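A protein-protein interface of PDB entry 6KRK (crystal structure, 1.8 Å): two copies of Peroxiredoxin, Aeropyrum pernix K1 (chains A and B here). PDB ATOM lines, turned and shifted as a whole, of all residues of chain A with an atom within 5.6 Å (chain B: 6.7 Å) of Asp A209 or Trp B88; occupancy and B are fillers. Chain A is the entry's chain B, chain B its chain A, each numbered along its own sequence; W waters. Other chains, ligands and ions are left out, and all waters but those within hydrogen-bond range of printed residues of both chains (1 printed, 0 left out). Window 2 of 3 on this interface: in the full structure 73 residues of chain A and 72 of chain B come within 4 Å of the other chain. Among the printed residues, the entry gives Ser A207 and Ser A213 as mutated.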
ATOM      1  N   MET A 200     -31.168  34.434  -9.259  1.00  0.00           N
ATOM      2  CA  MET A 200     -30.207  35.282  -8.521  1.00  0.00           C
ATOM      3  C   MET A 200     -30.835  36.649  -8.200  1.00  0.00           C
ATOM      4  O   MET A 200     -30.540  37.153  -7.124  1.00  0.00           O
ATOM      5  CB  MET A 200     -28.875  35.386  -9.264  1.00  0.00           C
ATOM      6  CG  MET A 200     -28.010  34.137  -9.031  1.00  0.00           C
ATOM      7  SD  MET A 200     -27.872  33.650  -7.245  1.00  0.00           S
ATOM      8  CE  MET A 200     -29.265  32.554  -6.981  1.00  0.00           C
ATOM      9  N   SER A 207     -29.099  30.781  -0.958  1.00  0.00           N
ATOM     10  CA  SER A 207     -28.352  30.362  -2.170  1.00  0.00           C
ATOM     11  C   SER A 207     -26.876  30.316  -1.857  1.00  0.00           C
ATOM     12  O   SER A 207     -26.378  31.251  -1.193  1.00  0.00           O
ATOM     13  CB  SER A 207     -28.563  31.318  -3.311  1.00  0.00           C
ATOM     14  OG  SER A 207     -29.314  30.682  -4.299  1.00  0.00           O
ATOM     15  N   LEU A 208     -26.171  29.347  -2.425  1.00  0.00           N
ATOM     16  CA  LEU A 208     -24.696  29.386  -2.434  1.00  0.00           C
ATOM     17  C   LEU A 208     -24.226  29.802  -3.832  1.00  0.00           C
ATOM     18  O   LEU A 208     -23.069  30.164  -3.964  1.00  0.00           O
ATOM     19  CB  LEU A 208     -24.148  28.007  -2.090  1.00  0.00           C
ATOM     20  CG  LEU A 208     -23.733  27.712  -0.649  1.00  0.00           C
ATOM     21  CD1 LEU A 208     -24.150  28.775   0.331  1.00  0.00           C
ATOM     22  CD2 LEU A 208     -24.208  26.329  -0.233  1.00  0.00           C
ATOM     23  N   ASP A 209     -25.054  29.588  -4.832  1.00  0.00           N
ATOM     24  CA  ASP A 209     -24.783  29.950  -6.246  1.00  0.00           C
ATOM     25  C   ASP A 209     -26.106  29.820  -6.968  1.00  0.00           C
ATOM     26  O   ASP A 209     -27.090  29.286  -6.339  1.00  0.00           O
ATOM     27  CB  ASP A 209     -23.649  29.117  -6.856  1.00  0.00           C
ATOM     28  CG  ASP A 209     -22.977  29.754  -8.081  1.00  0.00           C
ATOM     29  OD1 ASP A 209     -23.422  30.835  -8.503  1.00  0.00           O
ATOM     30  OD2 ASP A 209     -22.028  29.154  -8.601  1.00  0.00           O
ATOM     31  N   TRP A 210     -26.160  30.209  -8.251  1.00  0.00           N
ATOM     32  CA  TRP A 210     -27.425  30.205  -9.014  1.00  0.00           C
ATOM     33  C   TRP A 210     -27.945  28.774  -9.095  1.00  0.00           C
ATOM     34  O   TRP A 210     -29.140  28.608  -9.262  1.00  0.00           O
ATOM     35  CB  TRP A 210     -27.278  30.843 -10.410  1.00  0.00           C
ATOM     36  CG  TRP A 210     -26.222  30.210 -11.264  1.00  0.00           C
ATOM     37  CD1 TRP A 210     -24.918  30.604 -11.430  1.00  0.00           C
ATOM     38  CD2 TRP A 210     -26.387  29.016 -12.034  1.00  0.00           C
ATOM     39  NE1 TRP A 210     -24.268  29.731 -12.256  1.00  0.00           N
ATOM     40  CE2 TRP A 210     -25.155  28.774 -12.681  1.00  0.00           C
ATOM     41  CE3 TRP A 210     -27.482  28.190 -12.292  1.00  0.00           C
ATOM     42  CZ2 TRP A 210     -24.985  27.682 -13.533  1.00  0.00           C
ATOM     43  CZ3 TRP A 210     -27.319  27.136 -13.152  1.00  0.00           C
ATOM     44  CH2 TRP A 210     -26.078  26.876 -13.746  1.00  0.00           C
ATOM     45  N   TRP A 211     -27.057  27.781  -9.003  1.00  0.00           N
ATOM     46  CA  TRP A 211     -27.461  26.348  -9.165  1.00  0.00           C
ATOM     47  C   TRP A 211     -27.729  25.665  -7.807  1.00  0.00           C
ATOM     48  O   TRP A 211     -28.179  24.500  -7.812  1.00  0.00           O
ATOM     49  CB  TRP A 211     -26.408  25.604  -9.971  1.00  0.00           C
ATOM     50  CG  TRP A 211     -25.036  25.745  -9.402  1.00  0.00           C
ATOM     51  CD1 TRP A 211     -24.123  26.712  -9.736  1.00  0.00           C
ATOM     52  CD2 TRP A 211     -24.370  24.872  -8.488  1.00  0.00           C
ATOM     53  NE1 TRP A 211     -22.954  26.508  -9.065  1.00  0.00           N
ATOM     54  CE2 TRP A 211     -23.073  25.395  -8.286  1.00  0.00           C
ATOM     55  CE3 TRP A 211     -24.758  23.719  -7.782  1.00  0.00           C
ATOM     56  CZ2 TRP A 211     -22.142  24.811  -7.424  1.00  0.00           C
ATOM     57  CZ3 TRP A 211     -23.838  23.150  -6.938  1.00  0.00           C
ATOM     58  CH2 TRP A 211     -22.547  23.668  -6.776  1.00  0.00           C
ATOM     59  N   PHE A 212     -27.510  26.374  -6.696  1.00  0.00           N
ATOM     60  CA  PHE A 212     -27.613  25.808  -5.327  1.00  0.00           C
ATOM     61  C   PHE A 212     -28.446  26.753  -4.458  1.00  0.00           C
ATOM     62  O   PHE A 212     -27.859  27.574  -3.764  1.00  0.00           O
ATOM     63  CB  PHE A 212     -26.226  25.552  -4.744  1.00  0.00           C
ATOM     64  CG  PHE A 212     -26.218  24.603  -3.566  1.00  0.00           C
ATOM     65  CD1 PHE A 212     -27.249  24.556  -2.647  1.00  0.00           C
ATOM     66  CD2 PHE A 212     -25.149  23.749  -3.378  1.00  0.00           C
ATOM     67  CE1 PHE A 212     -27.205  23.658  -1.584  1.00  0.00           C
ATOM     68  CE2 PHE A 212     -25.098  22.864  -2.313  1.00  0.00           C
ATOM     69  CZ  PHE A 212     -26.131  22.825  -1.422  1.00  0.00           C
ATOM     70  N   SER A 213     -29.762  26.572  -4.517  1.00  0.00           N
ATOM     71  CA  SER A 213     -30.798  27.268  -3.714  1.00  0.00           C
ATOM     72  C   SER A 213     -31.584  26.242  -2.900  1.00  0.00           C
ATOM     73  O   SER A 213     -31.755  25.128  -3.335  1.00  0.00           O
ATOM     74  CB  SER A 213     -31.708  28.052  -4.564  1.00  0.00           C
ATOM     75  OG  SER A 213     -30.964  28.995  -5.335  1.00  0.00           O
ATOM     76  N   PHE B  46     -21.765  20.716 -10.757  1.00  0.00           N
ATOM     77  CA  PHE B  46     -22.506  21.970 -10.514  1.00  0.00           C
ATOM     78  C   PHE B  46     -23.999  21.682 -10.437  1.00  0.00           C
ATOM     79  O   PHE B  46     -24.799  22.476 -10.938  1.00  0.00           O
ATOM     80  CB  PHE B  46     -22.203  23.004 -11.610  1.00  0.00           C
ATOM     81  CG  PHE B  46     -20.756  23.399 -11.648  1.00  0.00           C
ATOM     82  CD1 PHE B  46     -20.230  24.248 -10.667  1.00  0.00           C
ATOM     83  CD2 PHE B  46     -19.941  23.015 -12.702  1.00  0.00           C
ATOM     84  CE1 PHE B  46     -18.909  24.669 -10.727  1.00  0.00           C
ATOM     85  CE2 PHE B  46     -18.622  23.450 -12.762  1.00  0.00           C
ATOM     86  CZ  PHE B  46     -18.111  24.239 -11.757  1.00  0.00           C
ATOM     87  N   THR B  51     -23.505  17.937  -5.021  1.00  0.00           N
ATOM     88  CA  THR B  51     -22.536  18.683  -4.196  1.00  0.00           C
ATOM     89  C   THR B  51     -22.697  18.261  -2.738  1.00  0.00           C
ATOM     90  O   THR B  51     -21.691  17.979  -2.100  1.00  0.00           O
ATOM     91  CB  THR B  51     -22.705  20.188  -4.384  1.00  0.00           C
ATOM     92  OG1 THR B  51     -22.449  20.491  -5.755  1.00  0.00           O
ATOM     93  CG2 THR B  51     -21.776  20.977  -3.496  1.00  0.00           C
ATOM     94  N   ILE B  83     -12.607  19.419 -12.171  1.00  0.00           N
ATOM     95  CA  ILE B  83     -11.583  20.201 -11.437  1.00  0.00           C
ATOM     96  C   ILE B  83     -12.229  21.520 -11.020  1.00  0.00           C
ATOM     97  O   ILE B  83     -12.037  21.927  -9.858  1.00  0.00           O
ATOM     98  CB  ILE B  83     -10.300  20.369 -12.276  1.00  0.00           C
ATOM     99  CG1 ILE B  83      -9.643  19.023 -12.572  1.00  0.00           C
ATOM    100  CG2 ILE B  83      -9.322  21.305 -11.627  1.00  0.00           C
ATOM    101  CD1 ILE B  83      -8.597  19.110 -13.648  1.00  0.00           C
ATOM    102  N   LYS B  84     -12.936  22.201 -11.923  1.00  0.00           N
ATOM    103  CA  LYS B  84     -13.579  23.504 -11.596  1.00  0.00           C
ATOM    104  C   LYS B  84     -14.638  23.314 -10.509  1.00  0.00           C
ATOM    105  O   LYS B  84     -14.733  24.169  -9.649  1.00  0.00           O
ATOM    106  CB  LYS B  84     -14.225  24.160 -12.810  1.00  0.00           C
ATOM    107  CG  LYS B  84     -13.241  24.793 -13.772  1.00  0.00           C
ATOM    108  CD  LYS B  84     -12.354  25.853 -13.194  1.00  0.00           C
ATOM    109  CE  LYS B  84     -13.008  27.186 -13.050  1.00  0.00           C
ATOM    110  NZ  LYS B  84     -12.106  28.138 -12.378  1.00  0.00           N
ATOM    111  N   TRP B  85     -15.396  22.214 -10.532  1.00  0.00           N
ATOM    112  CA  TRP B  85     -16.463  21.986  -9.533  1.00  0.00           C
ATOM    113  C   TRP B  85     -15.826  21.679  -8.174  1.00  0.00           C
ATOM    114  O   TRP B  85     -16.266  22.231  -7.163  1.00  0.00           O
ATOM    115  CB  TRP B  85     -17.359  20.849 -10.024  1.00  0.00           C
ATOM    116  CG  TRP B  85     -18.484  20.523  -9.110  1.00  0.00           C
ATOM    117  CD1 TRP B  85     -19.341  21.368  -8.497  1.00  0.00           C
ATOM    118  CD2 TRP B  85     -18.919  19.201  -8.787  1.00  0.00           C
ATOM    119  NE1 TRP B  85     -20.283  20.664  -7.794  1.00  0.00           N
ATOM    120  CE2 TRP B  85     -20.054  19.331  -7.976  1.00  0.00           C
ATOM    121  CE3 TRP B  85     -18.437  17.942  -9.123  1.00  0.00           C
ATOM    122  CZ2 TRP B  85     -20.722  18.225  -7.463  1.00  0.00           C
ATOM    123  CZ3 TRP B  85     -19.070  16.840  -8.594  1.00  0.00           C
ATOM    124  CH2 TRP B  85     -20.214  16.993  -7.801  1.00  0.00           C
ATOM    125  N   LYS B  86     -14.815  20.831  -8.130  1.00  0.00           N
ATOM    126  CA  LYS B  86     -14.119  20.544  -6.840  1.00  0.00           C
ATOM    127  C   LYS B  86     -13.488  21.834  -6.294  1.00  0.00           C
ATOM    128  O   LYS B  86     -13.498  22.044  -5.084  1.00  0.00           O
ATOM    129  CB  LYS B  86     -13.137  19.381  -7.001  1.00  0.00           C
ATOM    130  CG  LYS B  86     -13.800  18.015  -7.125  1.00  0.00           C
ATOM    131  CD  LYS B  86     -12.868  16.886  -7.542  1.00  0.00           C
ATOM    132  CE  LYS B  86     -11.644  16.701  -6.691  1.00  0.00           C
ATOM    133  NZ  LYS B  86     -10.980  15.409  -6.990  1.00  0.00           N
ATOM    134  N   GLU B  87     -12.951  22.700  -7.160  1.00  0.00           N
ATOM    135  CA  GLU B  87     -12.390  24.015  -6.751  1.00  0.00           C
ATOM    136  C   GLU B  87     -13.507  24.840  -6.115  1.00  0.00           C
ATOM    137  O   GLU B  87     -13.283  25.444  -5.062  1.00  0.00           O
ATOM    138  CB  GLU B  87     -11.794  24.638  -8.027  1.00  0.00           C
ATOM    139  CG  GLU B  87     -11.155  25.992  -7.917  1.00  0.00           C
ATOM    140  CD  GLU B  87     -10.607  26.482  -9.270  1.00  0.00           C
ATOM    141  OE1 GLU B  87     -10.564  25.662 -10.250  1.00  0.00           O
ATOM    142  OE2 GLU B  87     -10.250  27.688  -9.368  1.00  0.00           O
ATOM    143  N   TRP B  88     -14.679  24.856  -6.732  1.00  0.00           N
ATOM    144  CA  TRP B  88     -15.847  25.614  -6.250  1.00  0.00           C
ATOM    145  C   TRP B  88     -16.236  25.120  -4.850  1.00  0.00           C
ATOM    146  O   TRP B  88     -16.404  25.960  -3.956  1.00  0.00           O
ATOM    147  CB  TRP B  88     -17.037  25.511  -7.220  1.00  0.00           C
ATOM    148  CG  TRP B  88     -18.170  26.383  -6.777  1.00  0.00           C
ATOM    149  CD1 TRP B  88     -18.437  27.659  -7.181  1.00  0.00           C
ATOM    150  CD2 TRP B  88     -19.137  26.064  -5.768  1.00  0.00           C
ATOM    151  NE1 TRP B  88     -19.549  28.135  -6.533  1.00  0.00           N
ATOM    152  CE2 TRP B  88     -19.980  27.189  -5.642  1.00  0.00           C
ATOM    153  CE3 TRP B  88     -19.400  24.938  -4.988  1.00  0.00           C
ATOM    154  CZ2 TRP B  88     -21.060  27.202  -4.773  1.00  0.00           C
ATOM    155  CZ3 TRP B  88     -20.440  24.971  -4.089  1.00  0.00           C
ATOM    156  CH2 TRP B  88     -21.260  26.090  -3.996  1.00  0.00           C
ATOM    157  N   ILE B  89     -16.331  23.810  -4.664  1.00  0.00           N
ATOM    158  CA  ILE B  89     -16.661  23.215  -3.332  1.00  0.00           C
ATOM    159  C   ILE B  89     -15.625  23.648  -2.276  1.00  0.00           C
ATOM    160  O   ILE B  89     -16.017  24.050  -1.185  1.00  0.00           O
ATOM    161  CB  ILE B  89     -16.781  21.687  -3.451  1.00  0.00           C
ATOM    162  CG1 ILE B  89     -17.957  21.326  -4.376  1.00  0.00           C
ATOM    163  CG2 ILE B  89     -16.926  21.069  -2.069  1.00  0.00           C
ATOM    164  CD1 ILE B  89     -18.077  19.868  -4.743  1.00  0.00           C
ATOM    165  N   GLU B  90     -14.339  23.499  -2.549  1.00  0.00           N
ATOM    166  CA  GLU B  90     -13.273  23.902  -1.597  1.00  0.00           C
ATOM    167  C   GLU B  90     -13.403  25.406  -1.261  1.00  0.00           C
ATOM    168  O   GLU B  90     -13.425  25.768  -0.077  1.00  0.00           O
ATOM    169  CB  GLU B  90     -11.901  23.520  -2.157  1.00  0.00           C
ATOM    170  CG  GLU B  90     -10.780  23.845  -1.175  1.00  0.00           C
ATOM    171  CD  GLU B  90      -9.409  23.238  -1.454  1.00  0.00           C
ATOM    172  OE1 GLU B  90      -9.150  22.774  -2.602  1.00  0.00           O
ATOM    173  OE2 GLU B  90      -8.577  23.244  -0.511  1.00  0.00           O
ATOM    174  N   ARG B  91     -13.576  26.266  -2.257  1.00  0.00           N
ATOM    175  CA  ARG B  91     -13.640  27.745  -2.078  1.00  0.00           C
ATOM    176  C   ARG B  91     -14.927  28.182  -1.334  1.00  0.00           C
ATOM    177  O   ARG B  91     -14.820  29.017  -0.434  1.00  0.00           O
ATOM    178  CB  ARG B  91     -13.479  28.389  -3.463  1.00  0.00           C
ATOM    179  CG  ARG B  91     -13.202  29.888  -3.474  1.00  0.00           C
ATOM    180  CD  ARG B  91     -12.614  30.353  -4.810  1.00  0.00           C
ATOM    181  NE  ARG B  91     -13.066  31.687  -5.213  1.00  0.00           N
ATOM    182  CZ  ARG B  91     -14.132  31.965  -5.985  1.00  0.00           C
ATOM    183  NH1 ARG B  91     -14.912  31.005  -6.468  1.00  0.00           N
ATOM    184  NH2 ARG B  91     -14.418  33.226  -6.269  1.00  0.00           N
ATOM    185  N   HIS B  92     -16.111  27.688  -1.702  1.00  0.00           N
ATOM    186  CA  HIS B  92     -17.417  28.169  -1.183  1.00  0.00           C
ATOM    187  C   HIS B  92     -17.896  27.344   0.020  1.00  0.00           C
ATOM    188  O   HIS B  92     -18.664  27.896   0.811  1.00  0.00           O
ATOM    189  CB  HIS B  92     -18.461  28.203  -2.312  1.00  0.00           C
ATOM    190  CG  HIS B  92     -18.123  29.197  -3.369  1.00  0.00           C
ATOM    191  ND1 HIS B  92     -18.666  30.462  -3.386  1.00  0.00           N
ATOM    192  CD2 HIS B  92     -17.283  29.125  -4.433  1.00  0.00           C
ATOM    193  CE1 HIS B  92     -18.186  31.122  -4.423  1.00  0.00           C
ATOM    194  NE2 HIS B  92     -17.333  30.325  -5.085  1.00  0.00           N
ATOM    195  N   ILE B  93     -17.611  26.047   0.101  1.00  0.00           N
ATOM    196  CA  ILE B  93     -18.077  25.216   1.255  1.00  0.00           C
ATOM    197  C   ILE B  93     -16.905  24.987   2.208  1.00  0.00           C
ATOM    198  O   ILE B  93     -17.137  24.666   3.381  1.00  0.00           O
ATOM    199  CB  ILE B  93     -18.781  23.932   0.753  1.00  0.00           C
ATOM    200  CG1 ILE B  93     -20.002  24.298  -0.096  1.00  0.00           C
ATOM    201  CG2 ILE B  93     -19.194  23.024   1.901  1.00  0.00           C
ATOM    202  CD1 ILE B  93     -20.529  23.159  -0.887  1.00  0.00           C
ATOM    203  N   GLY B  94     -15.671  25.169   1.771  1.00  0.00           N
ATOM    204  CA  GLY B  94     -14.513  24.966   2.662  1.00  0.00           C
ATOM    205  C   GLY B  94     -14.199  23.499   2.873  1.00  0.00           C
ATOM    206  O   GLY B  94     -13.556  23.185   3.824  1.00  0.00           O
ATOM    207  N   VAL B  95     -14.611  22.612   1.972  1.00  0.00           N
ATOM    208  CA  VAL B  95     -14.342  21.159   2.133  1.00  0.00           C
ATOM    209  C   VAL B  95     -13.589  20.710   0.886  1.00  0.00           C
ATOM    210  O   VAL B  95     -14.107  20.904  -0.231  1.00  0.00           O
ATOM    211  CB  VAL B  95     -15.664  20.389   2.352  1.00  0.00           C
ATOM    212  CG1 VAL B  95     -15.451  18.876   2.360  1.00  0.00           C
ATOM    213  CG2 VAL B  95     -16.347  20.831   3.630  1.00  0.00           C
HETATM  214  O   HOH W   1     -21.030  30.614  -2.145  1.00  0.00           O
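NE1 of Trp B88 sits at hydrogen-bond distance from OD2 of Asp A209.
A ring nitrogen (NE2) of His B92 lies close to the indole nitrogen (NE1) of Trp B88. The indole nitrogen (NE1) of Trp A211 is in hydrogen-bond range of the side-chain carboxylate (OD2) of Asp A209 (2.8 Å). OG of Ser A207 lies close to O of Phe A212 (3.5 Å). The side-chain hydroxyl of Thr B51 sits at hydrogen-bond distance from the indole nitrogen of Trp B85, at 3.0 Å. The side-chain hydroxyl (OG) of Ser A207 is in hydrogen-bond range of the backbone carbonyl oxygen (O) of Asp A209 (3.3 Å).
Leu A208 touches Trp B88 (O to CZ2, 3.7 Å). O of Phe B46 touches CE3 of Trp A211 (3.4 Å). Trp A211 touches Thr B51 (CZ3 to OG1, 3.2 Å). Trp B85 touches Trp A211. Trp B88 touches Trp A211. CG2 of Thr B51 touches CE2 of Phe A212, 3.999 Å away.
Printed residues of chain B within 4 Å of Leu A208: Trp B88 (3.7 Å). Of chain B, only Trp B88 comes within 4 Å of Asp A209. Printed residues of chain B within 4 Å of Phe A212: Thr B51 (3.999 Å). Of the printed residues of chain A, Thr B51 touches Trp A211 and Phe A212. Trp B88 touches three residues of chain A. Ile B89 touches none of the printed residues of chain A. Val B95 touches none of the printed residues of chain A. The nearest residue of chain B that does not touch Asp A209 is Phe B46 (5.6 Å). The nearest printed residue of chain A that does not touch Trp B85 is Phe A212 (7.3 Å).
Of the 15 printed residues of chain B, 4 touch a printed residue of chain A. Hydrophobic or aromatic side chains of chain B within 4 Å of the printed part of chain A: Phe B46, Trp B85 and Trp B88. Hydrophobic or aromatic side chains of chain A that line the printed part of chain B: Leu A208, Trp A211 and Phe A212. Among the printed residues, 7 pairs touch across the chains. Among the printed residues, no Asp or Glu carboxylate lies within 4 Å of a Lys or Arg side-chain nitrogen of the other chain.
No position is printed for both chains.
Water W1 lies within hydrogen-bond range of a ring nitrogen (ND1) of His B92 (2.7 Å) and the backbone carbonyl oxygen (O) of Leu A208 (2.8 Å).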
